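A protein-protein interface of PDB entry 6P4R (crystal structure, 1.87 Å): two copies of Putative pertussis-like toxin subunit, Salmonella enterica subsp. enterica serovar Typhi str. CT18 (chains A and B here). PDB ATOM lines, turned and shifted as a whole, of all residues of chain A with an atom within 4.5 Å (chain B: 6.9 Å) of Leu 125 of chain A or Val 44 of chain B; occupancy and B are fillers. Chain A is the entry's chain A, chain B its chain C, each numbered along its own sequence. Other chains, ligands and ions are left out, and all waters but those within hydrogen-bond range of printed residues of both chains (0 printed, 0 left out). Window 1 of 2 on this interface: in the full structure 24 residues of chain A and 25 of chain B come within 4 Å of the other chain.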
ATOM      1  N   ILE A  55      15.120  31.398   1.608  1.00  0.00           N
ATOM      2  CA  ILE A  55      15.546  31.827   2.931  1.00  0.00           C
ATOM      3  C   ILE A  55      16.540  32.959   2.764  1.00  0.00           C
ATOM      4  O   ILE A  55      17.212  33.082   1.732  1.00  0.00           O
ATOM      5  CB  ILE A  55      16.173  30.687   3.752  1.00  0.00           C
ATOM      6  CG1 ILE A  55      17.290  29.979   2.970  1.00  0.00           C
ATOM      7  CG2 ILE A  55      15.083  29.693   4.171  1.00  0.00           C
ATOM      8  CD1 ILE A  55      18.037  28.924   3.803  1.00  0.00           C
ATOM      9  N   GLU A  84      13.331  17.806   2.159  1.00  0.00           N
ATOM     10  CA  GLU A  84      14.327  17.716   3.220  1.00  0.00           C
ATOM     11  C   GLU A  84      14.886  19.093   3.562  1.00  0.00           C
ATOM     12  O   GLU A  84      15.049  19.428   4.740  1.00  0.00           O
ATOM     13  CB  GLU A  84      15.464  16.773   2.813  1.00  0.00           C
ATOM     14  CG  GLU A  84      16.617  16.728   3.817  1.00  0.00           C
ATOM     15  CD  GLU A  84      17.643  15.604   3.578  1.00  0.00           C
ATOM     16  OE1 GLU A  84      17.489  14.775   2.669  1.00  0.00           O
ATOM     17  OE2 GLU A  84      18.617  15.530   4.346  1.00  0.00           O
ATOM     18  N   LEU A  85      15.211  19.892   2.535  1.00  0.00           N
ATOM     19  CA  LEU A  85      15.744  21.235   2.754  1.00  0.00           C
ATOM     20  C   LEU A  85      14.696  22.164   3.362  1.00  0.00           C
ATOM     21  O   LEU A  85      15.011  22.954   4.261  1.00  0.00           O
ATOM     22  CB  LEU A  85      16.268  21.809   1.428  1.00  0.00           C
ATOM     23  CG  LEU A  85      17.508  21.117   0.836  1.00  0.00           C
ATOM     24  CD1 LEU A  85      17.729  21.512  -0.639  1.00  0.00           C
ATOM     25  CD2 LEU A  85      18.750  21.410   1.654  1.00  0.00           C
ATOM     26  N   GLN A  88      14.270  21.220   7.019  1.00  0.00           N
ATOM     27  CA  GLN A  88      15.425  21.590   7.830  1.00  0.00           C
ATOM     28  C   GLN A  88      15.555  23.102   7.960  1.00  0.00           C
ATOM     29  O   GLN A  88      15.886  23.607   9.040  1.00  0.00           O
ATOM     30  CB  GLN A  88      16.700  20.988   7.248  1.00  0.00           C
ATOM     31  CG  GLN A  88      17.785  20.875   8.299  1.00  0.00           C
ATOM     32  CD  GLN A  88      17.341  20.022   9.464  1.00  0.00           C
ATOM     33  OE1 GLN A  88      16.885  18.886   9.276  1.00  0.00           O
ATOM     34  NE2 GLN A  88      17.470  20.555  10.682  1.00  0.00           N
ATOM     35  N   ALA A  89      15.287  23.840   6.872  1.00  0.00           N
ATOM     36  CA  ALA A  89      15.280  25.299   6.937  1.00  0.00           C
ATOM     37  C   ALA A  89      14.260  25.802   7.954  1.00  0.00           C
ATOM     38  O   ALA A  89      14.543  26.726   8.730  1.00  0.00           O
ATOM     39  CB  ALA A  89      14.999  25.888   5.549  1.00  0.00           C
ATOM     40  N   PHE A  92      15.737  25.214  11.562  1.00  0.00           N
ATOM     41  CA  PHE A  92      16.803  26.149  11.918  1.00  0.00           C
ATOM     42  C   PHE A  92      16.285  27.588  11.968  1.00  0.00           C
ATOM     43  O   PHE A  92      16.781  28.407  12.749  1.00  0.00           O
ATOM     44  CB  PHE A  92      17.969  26.036  10.931  1.00  0.00           C
ATOM     45  CG  PHE A  92      18.788  24.774  11.075  1.00  0.00           C
ATOM     46  CD1 PHE A  92      18.915  24.134  12.301  1.00  0.00           C
ATOM     47  CD2 PHE A  92      19.454  24.241   9.975  1.00  0.00           C
ATOM     48  CE1 PHE A  92      19.694  22.981  12.424  1.00  0.00           C
ATOM     49  CE2 PHE A  92      20.234  23.086  10.092  1.00  0.00           C
ATOM     50  CZ  PHE A  92      20.349  22.459  11.316  1.00  0.00           C
ATOM     51  N   ARG A 100      25.716  26.674   8.774  1.00  0.00           N
ATOM     52  CA  ARG A 100      26.414  26.943   7.526  1.00  0.00           C
ATOM     53  C   ARG A 100      25.433  26.700   6.384  1.00  0.00           C
ATOM     54  O   ARG A 100      24.776  25.654   6.339  1.00  0.00           O
ATOM     55  CB  ARG A 100      27.665  26.063   7.363  1.00  0.00           C
ATOM     56  CG  ARG A 100      28.353  26.230   5.986  1.00  0.00           C
ATOM     57  CD  ARG A 100      29.566  25.291   5.848  1.00  0.00           C
ATOM     58  NE  ARG A 100      30.650  25.708   6.749  1.00  0.00           N
ATOM     59  CZ  ARG A 100      31.551  24.883   7.279  1.00  0.00           C
ATOM     60  NH1 ARG A 100      31.525  23.600   6.986  1.00  0.00           N
ATOM     61  NH2 ARG A 100      32.485  25.343   8.103  1.00  0.00           N
ATOM     62  N   ILE A 101      25.300  27.674   5.498  1.00  0.00           N
ATOM     63  CA  ILE A 101      24.420  27.552   4.340  1.00  0.00           C
ATOM     64  C   ILE A 101      25.286  27.223   3.128  1.00  0.00           C
ATOM     65  O   ILE A 101      26.377  27.779   2.955  1.00  0.00           O
ATOM     66  CB  ILE A 101      23.569  28.826   4.138  1.00  0.00           C
ATOM     67  CG1 ILE A 101      22.665  28.696   2.912  1.00  0.00           C
ATOM     68  CG2 ILE A 101      24.420  30.093   4.058  1.00  0.00           C
ATOM     69  CD1 ILE A 101      21.682  29.860   2.720  1.00  0.00           C
ATOM     70  N   HIS A 102      24.829  26.273   2.321  1.00  0.00           N
ATOM     71  CA  HIS A 102      25.524  25.849   1.106  1.00  0.00           C
ATOM     72  C   HIS A 102      24.639  26.193  -0.082  1.00  0.00           C
ATOM     73  O   HIS A 102      23.445  25.869  -0.067  1.00  0.00           O
ATOM     74  CB  HIS A 102      25.802  24.338   1.126  1.00  0.00           C
ATOM     75  CG  HIS A 102      26.487  23.851   2.372  1.00  0.00           C
ATOM     76  ND1 HIS A 102      27.827  23.535   2.409  1.00  0.00           N
ATOM     77  CD2 HIS A 102      26.010  23.611   3.621  1.00  0.00           C
ATOM     78  CE1 HIS A 102      28.153  23.136   3.629  1.00  0.00           C
ATOM     79  NE2 HIS A 102      27.068  23.178   4.385  1.00  0.00           N
ATOM     80  N   LEU A 122      19.617  26.623  -3.028  1.00  0.00           N
ATOM     81  CA  LEU A 122      19.981  26.065  -1.736  1.00  0.00           C
ATOM     82  C   LEU A 122      20.321  24.593  -1.911  1.00  0.00           C
ATOM     83  O   LEU A 122      19.509  23.825  -2.438  1.00  0.00           O
ATOM     84  CB  LEU A 122      18.815  26.217  -0.761  1.00  0.00           C
ATOM     85  CG  LEU A 122      19.071  25.676   0.651  1.00  0.00           C
ATOM     86  CD1 LEU A 122      20.252  26.410   1.253  1.00  0.00           C
ATOM     87  CD2 LEU A 122      17.803  25.850   1.474  1.00  0.00           C
ATOM     88  N   GLY A 124      22.344  22.784   0.756  1.00  0.00           N
ATOM     89  CA  GLY A 124      22.599  22.096   2.009  1.00  0.00           C
ATOM     90  C   GLY A 124      22.537  23.050   3.185  1.00  0.00           C
ATOM     91  O   GLY A 124      22.683  24.267   3.034  1.00  0.00           O
ATOM     92  N   LEU A 125      22.301  22.470   4.367  1.00  0.00           N
ATOM     93  CA  LEU A 125      22.330  23.224   5.622  1.00  0.00           C
ATOM     94  C   LEU A 125      23.042  22.412   6.688  1.00  0.00           C
ATOM     95  O   LEU A 125      22.730  21.232   6.870  1.00  0.00           O
ATOM     96  CB  LEU A 125      20.920  23.551   6.114  1.00  0.00           C
ATOM     97  CG  LEU A 125      20.126  24.513   5.261  1.00  0.00           C
ATOM     98  CD1 LEU A 125      18.639  24.432   5.643  1.00  0.00           C
ATOM     99  CD2 LEU A 125      20.683  25.933   5.422  1.00  0.00           C
ATOM    100  N   SER A 126      23.956  23.046   7.420  1.00  0.00           N
ATOM    101  CA  SER A 126      24.773  22.379   8.428  1.00  0.00           C
ATOM    102  C   SER A 126      24.606  23.109   9.756  1.00  0.00           C
ATOM    103  O   SER A 126      24.680  24.337   9.793  1.00  0.00           O
ATOM    104  CB  SER A 126      26.253  22.371   8.016  1.00  0.00           C
ATOM    105  OG  SER A 126      26.474  21.743   6.758  1.00  0.00           O
ATOM    106  N   SER A 127      24.389  22.365  10.838  1.00  0.00           N
ATOM    107  CA  SER A 127      24.408  22.997  12.160  1.00  0.00           C
ATOM    108  C   SER A 127      25.836  23.415  12.507  1.00  0.00           C
ATOM    109  O   SER A 127      26.810  22.861  11.985  1.00  0.00           O
ATOM    110  CB  SER A 127      23.846  22.050  13.225  1.00  0.00           C
ATOM    111  OG  SER A 127      24.614  20.863  13.354  1.00  0.00           O
ATOM    112  N   LEU B  42      23.592  18.152  13.180  1.00  0.00           N
ATOM    113  CA  LEU B  42      22.781  17.578  12.114  1.00  0.00           C
ATOM    114  C   LEU B  42      23.031  18.367  10.835  1.00  0.00           C
ATOM    115  O   LEU B  42      23.107  19.598  10.863  1.00  0.00           O
ATOM    116  CB  LEU B  42      21.284  17.594  12.480  1.00  0.00           C
ATOM    117  CG  LEU B  42      20.391  16.727  11.576  1.00  0.00           C
ATOM    118  CD1 LEU B  42      19.321  15.999  12.376  1.00  0.00           C
ATOM    119  CD2 LEU B  42      19.754  17.592  10.536  1.00  0.00           C
ATOM    120  N   HIS B  43      23.150  17.648   9.717  1.00  0.00           N
ATOM    121  CA  HIS B  43      23.448  18.227   8.415  1.00  0.00           C
ATOM    122  C   HIS B  43      22.531  17.588   7.385  1.00  0.00           C
ATOM    123  O   HIS B  43      22.289  16.379   7.437  1.00  0.00           O
ATOM    124  CB  HIS B  43      24.920  17.969   8.043  1.00  0.00           C
ATOM    125  CG  HIS B  43      25.219  18.111   6.585  1.00  0.00           C
ATOM    126  ND1 HIS B  43      25.712  19.276   6.043  1.00  0.00           N
ATOM    127  CD2 HIS B  43      25.116  17.230   5.562  1.00  0.00           C
ATOM    128  CE1 HIS B  43      25.894  19.111   4.741  1.00  0.00           C
ATOM    129  NE2 HIS B  43      25.544  17.876   4.426  1.00  0.00           N
ATOM    130  N   VAL B  44      22.027  18.378   6.440  1.00  0.00           N
ATOM    131  CA  VAL B  44      21.277  17.816   5.321  1.00  0.00           C
ATOM    132  C   VAL B  44      21.917  18.255   4.012  1.00  0.00           C
ATOM    133  O   VAL B  44      22.381  19.394   3.886  1.00  0.00           O
ATOM    134  CB  VAL B  44      19.786  18.205   5.353  1.00  0.00           C
ATOM    135  CG1 VAL B  44      19.125  17.644   6.628  1.00  0.00           C
ATOM    136  CG2 VAL B  44      19.607  19.710   5.260  1.00  0.00           C
ATOM    137  N   GLY B  45      21.939  17.348   3.039  1.00  0.00           N
ATOM    138  CA  GLY B  45      22.469  17.665   1.739  1.00  0.00           C
ATOM    139  C   GLY B  45      21.935  16.726   0.667  1.00  0.00           C
ATOM    140  O   GLY B  45      20.925  16.045   0.855  1.00  0.00           O
ATOM    141  N   GLN B  46      22.645  16.695  -0.452  1.00  0.00           N
ATOM    142  CA  GLN B  46      22.343  15.785  -1.560  1.00  0.00           C
ATOM    143  C   GLN B  46      23.651  15.316  -2.173  1.00  0.00           C
ATOM    144  O   GLN B  46      24.612  16.084  -2.259  1.00  0.00           O
ATOM    145  CB  GLN B  46      21.483  16.469  -2.636  1.00  0.00           C
ATOM    146  CG  GLN B  46      21.036  15.518  -3.740  1.00  0.00           C
ATOM    147  CD  GLN B  46      20.065  16.143  -4.714  1.00  0.00           C
ATOM    148  OE1 GLN B  46      18.976  16.573  -4.336  1.00  0.00           O
ATOM    149  NE2 GLN B  46      20.457  16.196  -5.978  1.00  0.00           N
ATOM    150  N   TYR B  52      20.516  13.186   1.487  1.00  0.00           N
ATOM    151  CA  TYR B  52      21.165  12.477   2.582  1.00  0.00           C
ATOM    152  C   TYR B  52      21.173  13.375   3.811  1.00  0.00           C
ATOM    153  O   TYR B  52      21.013  14.589   3.712  1.00  0.00           O
ATOM    154  CB  TYR B  52      22.607  12.043   2.233  1.00  0.00           C
ATOM    155  CG  TYR B  52      23.626  13.170   2.261  1.00  0.00           C
ATOM    156  CD1 TYR B  52      23.915  13.897   1.105  1.00  0.00           C
ATOM    157  CD2 TYR B  52      24.299  13.513   3.448  1.00  0.00           C
ATOM    158  CE1 TYR B  52      24.841  14.935   1.114  1.00  0.00           C
ATOM    159  CE2 TYR B  52      25.213  14.552   3.466  1.00  0.00           C
ATOM    160  CZ  TYR B  52      25.480  15.262   2.295  1.00  0.00           C
ATOM    161  OH  TYR B  52      26.390  16.307   2.313  1.00  0.00           O
ATOM    162  N   PHE B  53      21.396  12.768   4.972  1.00  0.00           N
ATOM    163  CA  PHE B  53      21.645  13.550   6.178  1.00  0.00           C
ATOM    164  C   PHE B  53      22.725  12.867   7.000  1.00  0.00           C
ATOM    165  O   PHE B  53      22.951  11.662   6.886  1.00  0.00           O
ATOM    166  CB  PHE B  53      20.357  13.751   6.990  1.00  0.00           C
ATOM    167  CG  PHE B  53      19.924  12.546   7.793  1.00  0.00           C
ATOM    168  CD1 PHE B  53      19.137  11.548   7.221  1.00  0.00           C
ATOM    169  CD2 PHE B  53      20.260  12.432   9.132  1.00  0.00           C
ATOM    170  CE1 PHE B  53      18.723  10.432   7.971  1.00  0.00           C
ATOM    171  CE2 PHE B  53      19.835  11.323   9.888  1.00  0.00           C
ATOM    172  CZ  PHE B  53      19.070  10.322   9.297  1.00  0.00           C
ATOM    173  N   CYS B  54      23.395  13.650   7.850  1.00  0.00           N
ATOM    174  CA  CYS B  54      24.379  13.100   8.766  1.00  0.00           C
ATOM    175  C   CYS B  54      24.118  13.653  10.154  1.00  0.00           C
ATOM    176  O   CYS B  54      23.613  14.762  10.307  1.00  0.00           O
ATOM    177  CB  CYS B  54      25.821  13.444   8.357  1.00  0.00           C
ATOM    178  SG  CYS B  54      26.280  12.925   6.680  1.00  0.00           S
ATOM    179  N   LEU B  86      15.569   9.917   9.631  1.00  0.00           N
ATOM    180  CA  LEU B  86      15.748  11.374   9.628  1.00  0.00           C
ATOM    181  C   LEU B  86      14.807  12.030  10.633  1.00  0.00           C
ATOM    182  O   LEU B  86      15.218  12.872  11.447  1.00  0.00           O
ATOM    183  CB  LEU B  86      15.516  11.938   8.213  1.00  0.00           C
ATOM    184  CG  LEU B  86      15.458  13.466   8.016  1.00  0.00           C
ATOM    185  CD1 LEU B  86      16.713  14.133   8.563  1.00  0.00           C
ATOM    186  CD2 LEU B  86      15.257  13.839   6.517  1.00  0.00           C
ATOM    187  N   ARG B  90      15.961  13.893  14.073  1.00  0.00           N
ATOM    188  CA  ARG B  90      15.514  15.249  14.372  1.00  0.00           C
ATOM    189  C   ARG B  90      14.862  15.328  15.748  1.00  0.00           C
ATOM    190  O   ARG B  90      15.125  16.259  16.519  1.00  0.00           O
ATOM    191  CB  ARG B  90      14.544  15.727  13.284  1.00  0.00           C
ATOM    192  CG  ARG B  90      15.212  16.176  12.005  1.00  0.00           C
ATOM    193  CD  ARG B  90      14.167  16.550  10.921  1.00  0.00           C
ATOM    194  NE  ARG B  90      14.793  17.129   9.729  1.00  0.00           N
ATOM    195  CZ  ARG B  90      14.291  17.044   8.498  1.00  0.00           C
ATOM    196  NH1 ARG B  90      13.143  16.399   8.283  1.00  0.00           N
ATOM    197  NH2 ARG B  90      14.942  17.602   7.478  1.00  0.00           N
ATOM    198  N   PHE B 117      32.574  13.537   6.935  1.00  0.00           N
ATOM    199  CA  PHE B 117      31.614  12.919   7.828  1.00  0.00           C
ATOM    200  C   PHE B 117      32.221  11.599   8.276  1.00  0.00           C
ATOM    201  O   PHE B 117      33.106  11.588   9.146  1.00  0.00           O
ATOM    202  CB  PHE B 117      30.255  12.767   7.131  1.00  0.00           C
ATOM    203  CG  PHE B 117      29.590  14.086   6.753  1.00  0.00           C
ATOM    204  CD1 PHE B 117      29.187  14.985   7.732  1.00  0.00           C
ATOM    205  CD2 PHE B 117      29.332  14.394   5.418  1.00  0.00           C
ATOM    206  CE1 PHE B 117      28.540  16.204   7.384  1.00  0.00           C
ATOM    207  CE2 PHE B 117      28.696  15.595   5.062  1.00  0.00           C
ATOM    208  CZ  PHE B 117      28.302  16.500   6.053  1.00  0.00           C
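The side-chain carboxylate of Glu 84 of chain A lies close to the backbone carbonyl oxygen of Tyr 52 of chain B, 2.7 Å away.
The backbone NH (N) of Leu 42 of chain B is in hydrogen-bond range of the side-chain hydroxyl (OG) of Ser 127 of chain A, at 2.9 Å.
OG of Ser 126 of chain A sits at hydrogen-bond distance from ND1 of His 43 of chain B, at 2.7 Å.
O of Leu 125 of chain A sits at hydrogen-bond distance from N of Val 44 of chain B, 3.0 Å away.
The backbone carbonyl oxygen (O) of Glu 84 of chain A is in hydrogen-bond range of the guanidinium group (NH2) of Arg 90 of chain B, 3.3 Å away.
The guanidinium group (NE) of Arg 90 of chain B is in hydrogen-bond range of the side-chain amide oxygen (OE1) of Gln 88 of chain A.
OH of Tyr 52 of chain B sits at hydrogen-bond distance from NE2 of His 43 of chain B (2.8 Å).
N of Arg 100 of chain A lies within hydrogen-bond range of O of Ser 126 of chain A (2.8 Å).
The backbone NH (N) of His 102 of chain A sits at hydrogen-bond distance from the backbone carbonyl oxygen (O) of Gly 124 of chain A, at 3.0 Å.
The side-chain hydroxyl (OG) of Ser 126 of chain A is in hydrogen-bond range of a ring nitrogen (NE2) of His 102 of chain A (2.8 Å).
O of Gly 45 of chain B lies within hydrogen-bond range of N of Tyr 52 of chain B.
O of His 43 of chain B sits at hydrogen-bond distance from N of Cys 54 of chain B (3.0 Å).
OE2 of Glu 84 of chain A touches CB of Val 44 of chain B, at 3.1 Å.
Phe 53 of chain B touches Glu 84 of chain A (CB to OE2, 3.6 Å).
Gln 88 of chain A touches Leu 42 of chain B (OE1 to CD2, 3.4 Å).
Gln 88 of chain A touches Val 44 of chain B.
Phe 92 of chain A touches Leu 42 of chain B.
Val 44 of chain B touches Gly 124 of chain A (O to CA, 3.3 Å).
O of Leu 125 of chain A touches CA of His 43 of chain B, 3.5 Å away.
Ser 126 of chain A touches Leu 42 of chain B (C to O, 3.97 Å).
Leu 125 of chain A touches just these residues of chain B: His 43 and Val 44.
Printed residues of chain A within 4 Å of Val 44 of chain B: Glu 84 (3.1 Å), Gln 88 (3.7 Å), Gly 124 (3.3 Å) and Leu 125 (3.0 Å).
Of the printed residues of chain B, Phe 92 of chain A touches Leu 42 (3.9996 Å).
Of the printed residues of chain A, Tyr 52 of chain B touches Glu 84.
Of the printed residues of chain A, Phe 53 of chain B touches Glu 84.
Printed residues of chain A within 4 Å of Leu 42 of chain B: Gln 88 (3.4 Å), Phe 92 (3.9996 Å), Ser 126 (3.97 Å) and Ser 127 (2.9 Å).
Gly 45 of chain B touches none of the printed residues of chain A.
Leu 122 of chain A touches none of the printed residues of chain B.
The nearest residue of chain A that does not touch Val 44 of chain B is Leu 85 of chain A (4.1 Å).
Hydrophobic or aromatic side chains of chain A that line the printed part of chain B: Phe 92.
Of the 11 printed residues of chain B, 6 touch a printed residue of chain A.
Printed residues of chain B that touch a printed residue of chain A: Leu 42, His 43, Val 44, Tyr 52, Phe 53 and Arg 90.
Hydrophobic or aromatic side chains of chain B that line the printed part of chain A: Leu 42, His 43, Val 44 and Phe 53.
No position is printed for both chains.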
